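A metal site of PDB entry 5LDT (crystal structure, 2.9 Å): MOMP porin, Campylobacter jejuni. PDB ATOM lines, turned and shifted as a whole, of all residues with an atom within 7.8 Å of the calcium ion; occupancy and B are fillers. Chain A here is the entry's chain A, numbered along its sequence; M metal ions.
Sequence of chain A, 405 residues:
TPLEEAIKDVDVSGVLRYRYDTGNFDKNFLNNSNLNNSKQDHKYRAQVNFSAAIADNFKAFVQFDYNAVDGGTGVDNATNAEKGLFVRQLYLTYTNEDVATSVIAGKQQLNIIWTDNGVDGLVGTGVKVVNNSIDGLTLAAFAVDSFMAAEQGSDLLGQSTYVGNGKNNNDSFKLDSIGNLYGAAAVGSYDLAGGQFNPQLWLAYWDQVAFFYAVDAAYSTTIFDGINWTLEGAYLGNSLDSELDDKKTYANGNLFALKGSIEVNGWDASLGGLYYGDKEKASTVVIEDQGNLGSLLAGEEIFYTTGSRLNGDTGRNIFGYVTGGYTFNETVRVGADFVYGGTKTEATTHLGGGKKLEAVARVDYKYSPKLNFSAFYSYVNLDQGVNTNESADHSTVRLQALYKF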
ATOM      1  N   ARG A  45     -27.663  25.208  38.560  1.00  0.00           N
ATOM      2  CA  ARG A  45     -27.576  26.440  37.793  1.00  0.00           C
ATOM      3  C   ARG A  45     -28.872  27.179  37.938  1.00  0.00           C
ATOM      4  O   ARG A  45     -29.896  26.676  37.513  1.00  0.00           O
ATOM      5  CB  ARG A  45     -27.244  26.183  36.304  1.00  0.00           C
ATOM      6  CG  ARG A  45     -26.897  27.435  35.473  1.00  0.00           C
ATOM      7  CD  ARG A  45     -25.620  28.099  35.963  1.00  0.00           C
ATOM      8  NE  ARG A  45     -25.231  29.259  35.157  1.00  0.00           N
ATOM      9  CZ  ARG A  45     -24.488  29.256  34.046  1.00  0.00           C
ATOM     10  NH1 ARG A  45     -24.044  28.134  33.523  1.00  0.00           N
ATOM     11  NH2 ARG A  45     -24.169  30.413  33.446  1.00  0.00           N
ATOM     12  N   ARG A  88     -24.777  38.786  36.397  1.00  0.00           N
ATOM     13  CA  ARG A  88     -24.329  38.217  35.132  1.00  0.00           C
ATOM     14  C   ARG A  88     -24.644  39.107  33.908  1.00  0.00           C
ATOM     15  O   ARG A  88     -23.914  39.128  32.932  1.00  0.00           O
ATOM     16  CB  ARG A  88     -25.048  36.882  34.907  1.00  0.00           C
ATOM     17  CG  ARG A  88     -24.527  36.088  33.747  1.00  0.00           C
ATOM     18  CD  ARG A  88     -24.932  34.632  33.821  1.00  0.00           C
ATOM     19  NE  ARG A  88     -24.218  33.862  32.830  1.00  0.00           N
ATOM     20  CZ  ARG A  88     -24.577  33.667  31.549  1.00  0.00           C
ATOM     21  NH1 ARG A  88     -25.672  34.205  31.034  1.00  0.00           N
ATOM     22  NH2 ARG A  88     -23.803  32.883  30.772  1.00  0.00           N
ATOM     23  N   THR A 115     -22.652  31.813  19.230  1.00  0.00           N
ATOM     24  CA  THR A 115     -22.625  31.580  20.674  1.00  0.00           C
ATOM     25  C   THR A 115     -23.886  30.840  21.152  1.00  0.00           C
ATOM     26  O   THR A 115     -24.942  30.880  20.553  1.00  0.00           O
ATOM     27  CB  THR A 115     -22.508  32.893  21.479  1.00  0.00           C
ATOM     28  OG1 THR A 115     -23.646  33.720  21.245  1.00  0.00           O
ATOM     29  CG2 THR A 115     -21.255  33.638  21.104  1.00  0.00           C
ATOM     30  N   ASP A 116     -23.736  30.173  22.271  1.00  0.00           N
ATOM     31  CA  ASP A 116     -24.868  29.541  22.944  1.00  0.00           C
ATOM     32  C   ASP A 116     -25.877  30.669  23.275  1.00  0.00           C
ATOM     33  O   ASP A 116     -25.531  31.748  23.791  1.00  0.00           O
ATOM     34  CB  ASP A 116     -24.350  28.729  24.150  1.00  0.00           C
ATOM     35  CG  ASP A 116     -25.420  28.002  24.905  1.00  0.00           C
ATOM     36  OD1 ASP A 116     -26.572  27.969  24.461  1.00  0.00           O
ATOM     37  OD2 ASP A 116     -25.070  27.452  25.980  1.00  0.00           O
ATOM     38  N   GLY A 118     -28.662  29.829  25.091  1.00  0.00           N
ATOM     39  CA  GLY A 118     -29.402  29.306  26.247  1.00  0.00           C
ATOM     40  C   GLY A 118     -28.835  29.733  27.569  1.00  0.00           C
ATOM     41  O   GLY A 118     -28.252  30.840  27.695  1.00  0.00           O
ATOM     42  N   VAL A 119     -28.948  28.869  28.568  1.00  0.00           N
ATOM     43  CA  VAL A 119     -28.522  29.217  29.924  1.00  0.00           C
ATOM     44  C   VAL A 119     -27.061  29.766  30.012  1.00  0.00           C
ATOM     45  O   VAL A 119     -26.806  30.799  30.608  1.00  0.00           O
ATOM     46  CB  VAL A 119     -28.732  28.023  30.845  1.00  0.00           C
ATOM     47  CG1 VAL A 119     -28.071  28.230  32.187  1.00  0.00           C
ATOM     48  CG2 VAL A 119     -30.210  27.743  30.997  1.00  0.00           C
ATOM     49  N   ASP A 120     -26.124  29.056  29.370  1.00  0.00           N
ATOM     50  CA  ASP A 120     -24.684  29.333  29.518  1.00  0.00           C
ATOM     51  C   ASP A 120     -24.097  30.044  28.252  1.00  0.00           C
ATOM     52  O   ASP A 120     -22.989  29.753  27.856  1.00  0.00           O
ATOM     53  CB  ASP A 120     -23.941  28.036  29.806  1.00  0.00           C
ATOM     54  CG  ASP A 120     -22.582  28.248  30.387  1.00  0.00           C
ATOM     55  OD1 ASP A 120     -22.456  29.061  31.252  1.00  0.00           O
ATOM     56  OD2 ASP A 120     -21.592  27.574  30.041  1.00  0.00           O
ATOM     57  N   GLY A 121     -24.848  31.005  27.709  1.00  0.00           N
ATOM     58  CA  GLY A 121     -24.433  31.767  26.530  1.00  0.00           C
ATOM     59  C   GLY A 121     -23.428  32.865  26.854  1.00  0.00           C
ATOM     60  O   GLY A 121     -23.448  33.431  27.960  1.00  0.00           O
ATOM     61  N   LEU A 122     -22.526  33.139  25.914  1.00  0.00           N
ATOM     62  CA  LEU A 122     -21.472  34.103  26.141  1.00  0.00           C
ATOM     63  C   LEU A 122     -22.037  35.472  26.371  1.00  0.00           C
ATOM     64  O   LEU A 122     -22.953  35.905  25.651  1.00  0.00           O
ATOM     65  CB  LEU A 122     -20.471  34.149  24.980  1.00  0.00           C
ATOM     66  CG  LEU A 122     -19.332  35.175  25.077  1.00  0.00           C
ATOM     67  CD1 LEU A 122     -18.341  34.780  26.165  1.00  0.00           C
ATOM     68  CD2 LEU A 122     -18.594  35.293  23.746  1.00  0.00           C
ATOM     69  N   GLU A 151     -15.776  33.130  32.967  1.00  0.00           N
ATOM     70  CA  GLU A 151     -16.969  32.341  33.247  1.00  0.00           C
ATOM     71  C   GLU A 151     -17.137  31.173  32.262  1.00  0.00           C
ATOM     72  O   GLU A 151     -17.710  30.126  32.598  1.00  0.00           O
ATOM     73  CB  GLU A 151     -18.241  33.201  33.117  1.00  0.00           C
ATOM     74  CG  GLU A 151     -19.505  32.573  33.711  1.00  0.00           C
ATOM     75  CD  GLU A 151     -20.814  32.904  32.986  1.00  0.00           C
ATOM     76  OE1 GLU A 151     -20.864  32.981  31.732  1.00  0.00           O
ATOM     77  OE2 GLU A 151     -21.854  32.979  33.685  1.00  0.00           O
ATOM     78  N   GLN A 152     -16.743  31.396  31.017  1.00  0.00           N
ATOM     79  CA  GLN A 152     -16.927  30.430  29.965  1.00  0.00           C
ATOM     80  C   GLN A 152     -15.828  29.363  29.890  1.00  0.00           C
ATOM     81  O   GLN A 152     -16.053  28.280  29.305  1.00  0.00           O
ATOM     82  CB  GLN A 152     -17.099  31.188  28.643  1.00  0.00           C
ATOM     83  CG  GLN A 152     -18.412  31.954  28.596  1.00  0.00           C
ATOM     84  CD  GLN A 152     -19.601  31.013  28.707  1.00  0.00           C
ATOM     85  OE1 GLN A 152     -19.566  29.898  28.155  1.00  0.00           O
ATOM     86  NE2 GLN A 152     -20.664  31.439  29.370  1.00  0.00           N
ATOM     87  N   GLY A 153     -14.668  29.601  30.509  1.00  0.00           N
ATOM     88  CA  GLY A 153     -13.629  28.622  30.575  1.00  0.00           C
ATOM     89  C   GLY A 153     -13.319  28.129  29.187  1.00  0.00           C
ATOM     90  O   GLY A 153     -13.073  28.896  28.309  1.00  0.00           O
ATOM     91  N   SER A 154     -13.447  26.823  28.972  1.00  0.00           N
ATOM     92  CA  SER A 154     -13.055  26.188  27.723  1.00  0.00           C
ATOM     93  C   SER A 154     -14.167  26.234  26.668  1.00  0.00           C
ATOM     94  O   SER A 154     -13.943  25.796  25.537  1.00  0.00           O
ATOM     95  CB  SER A 154     -12.558  24.761  27.952  1.00  0.00           C
ATOM     96  OG  SER A 154     -13.617  23.882  28.256  1.00  0.00           O
ATOM     97  N   ASP A 155     -15.341  26.775  27.017  1.00  0.00           N
ATOM     98  CA  ASP A 155     -16.375  27.021  26.028  1.00  0.00           C
ATOM     99  C   ASP A 155     -15.904  28.107  25.023  1.00  0.00           C
ATOM    100  O   ASP A 155     -16.310  28.103  23.858  1.00  0.00           O
ATOM    101  CB  ASP A 155     -17.703  27.458  26.658  1.00  0.00           C
ATOM    102  CG  ASP A 155     -18.568  26.296  27.141  1.00  0.00           C
ATOM    103  OD1 ASP A 155     -18.093  25.176  27.391  1.00  0.00           O
ATOM    104  OD2 ASP A 155     -19.775  26.528  27.281  1.00  0.00           O
ATOM    105  N   LEU A 156     -15.016  28.999  25.455  1.00  0.00           N
ATOM    106  CA  LEU A 156     -14.630  30.065  24.566  1.00  0.00           C
ATOM    107  C   LEU A 156     -13.493  29.664  23.675  1.00  0.00           C
ATOM    108  O   LEU A 156     -12.507  29.060  24.122  1.00  0.00           O
ATOM    109  CB  LEU A 156     -14.242  31.311  25.376  1.00  0.00           C
ATOM    110  CG  LEU A 156     -14.020  32.596  24.561  1.00  0.00           C
ATOM    111  CD1 LEU A 156     -15.289  33.095  23.917  1.00  0.00           C
ATOM    112  CD2 LEU A 156     -13.483  33.677  25.483  1.00  0.00           C
ATOM    113  N   GLU A 288     -18.212  30.545  20.874  1.00  0.00           N
ATOM    114  CA  GLU A 288     -18.428  29.886  22.138  1.00  0.00           C
ATOM    115  C   GLU A 288     -19.252  28.582  21.987  1.00  0.00           C
ATOM    116  O   GLU A 288     -20.316  28.584  21.378  1.00  0.00           O
ATOM    117  CB  GLU A 288     -19.126  30.860  23.067  1.00  0.00           C
ATOM    118  CG  GLU A 288     -19.342  30.326  24.487  1.00  0.00           C
ATOM    119  CD  GLU A 288     -20.784  29.883  24.796  1.00  0.00           C
ATOM    120  OE1 GLU A 288     -21.702  30.559  24.314  1.00  0.00           O
ATOM    121  OE2 GLU A 288     -20.964  28.960  25.611  1.00  0.00           O
ATOM    122  N   ASP A 289     -18.719  27.515  22.587  1.00  0.00           N
ATOM    123  CA  ASP A 289     -19.299  26.186  22.697  1.00  0.00           C
ATOM    124  C   ASP A 289     -19.664  25.566  21.342  1.00  0.00           C
ATOM    125  O   ASP A 289     -18.756  25.136  20.627  1.00  0.00           O
ATOM    126  CB  ASP A 289     -20.426  26.085  23.759  1.00  0.00           C
ATOM    127  CG  ASP A 289     -20.710  24.592  24.234  1.00  0.00           C
ATOM    128  OD1 ASP A 289     -20.266  23.569  23.592  1.00  0.00           O
ATOM    129  OD2 ASP A 289     -21.429  24.440  25.256  1.00  0.00           O
ATOM    130  N   GLN A 290     -20.960  25.481  21.015  1.00  0.00           N
ATOM    131  CA  GLN A 290     -21.381  25.021  19.691  1.00  0.00           C
ATOM    132  C   GLN A 290     -22.294  26.044  19.039  1.00  0.00           C
ATOM    133  O   GLN A 290     -23.142  25.702  18.218  1.00  0.00           O
ATOM    134  CB  GLN A 290     -22.086  23.678  19.860  1.00  0.00           C
ATOM    135  CG  GLN A 290     -21.220  22.668  20.593  1.00  0.00           C
ATOM    136  CD  GLN A 290     -21.858  21.306  20.747  1.00  0.00           C
ATOM    137  OE1 GLN A 290     -23.028  21.194  21.120  1.00  0.00           O
ATOM    138  NE2 GLN A 290     -21.044  20.261  20.541  1.00  0.00           N
HETATM  139 CA    CA M   1     -21.171  28.286  27.819  1.00  0.00          CA
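OE1 of Glu 151 lies within hydrogen-bond range of NE2 of Gln 152, at 2.8 Å.
The backbone carbonyl oxygen of Asp 155 is in hydrogen-bond range of the backbone NH of Asp 289 (2.8 Å).
N of Leu 122 lies within hydrogen-bond range of OE1 of Glu 288 (3.1 Å).
The side-chain carboxylate (OE1) of Glu 288 is in hydrogen-bond range of the backbone NH (N) of Asp 116 (2.9 Å).
The guanidinium group of Arg 45 lies within salt-bridge range of the side-chain carboxylate of Asp 120 (2.9 Å).
Within 4 Å of the calcium ion: Asp 120, Gln 152, Asp 155 and Glu 288.
The nearest printed residue that does not touch the calcium ion is Asp 116 (4.4 Å).
The calcium ion is bound by OE1 of Gln 152, OD2 of Asp 155, OE2 of Glu 288, O of Asp 120 and OD2 of Asp 120.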
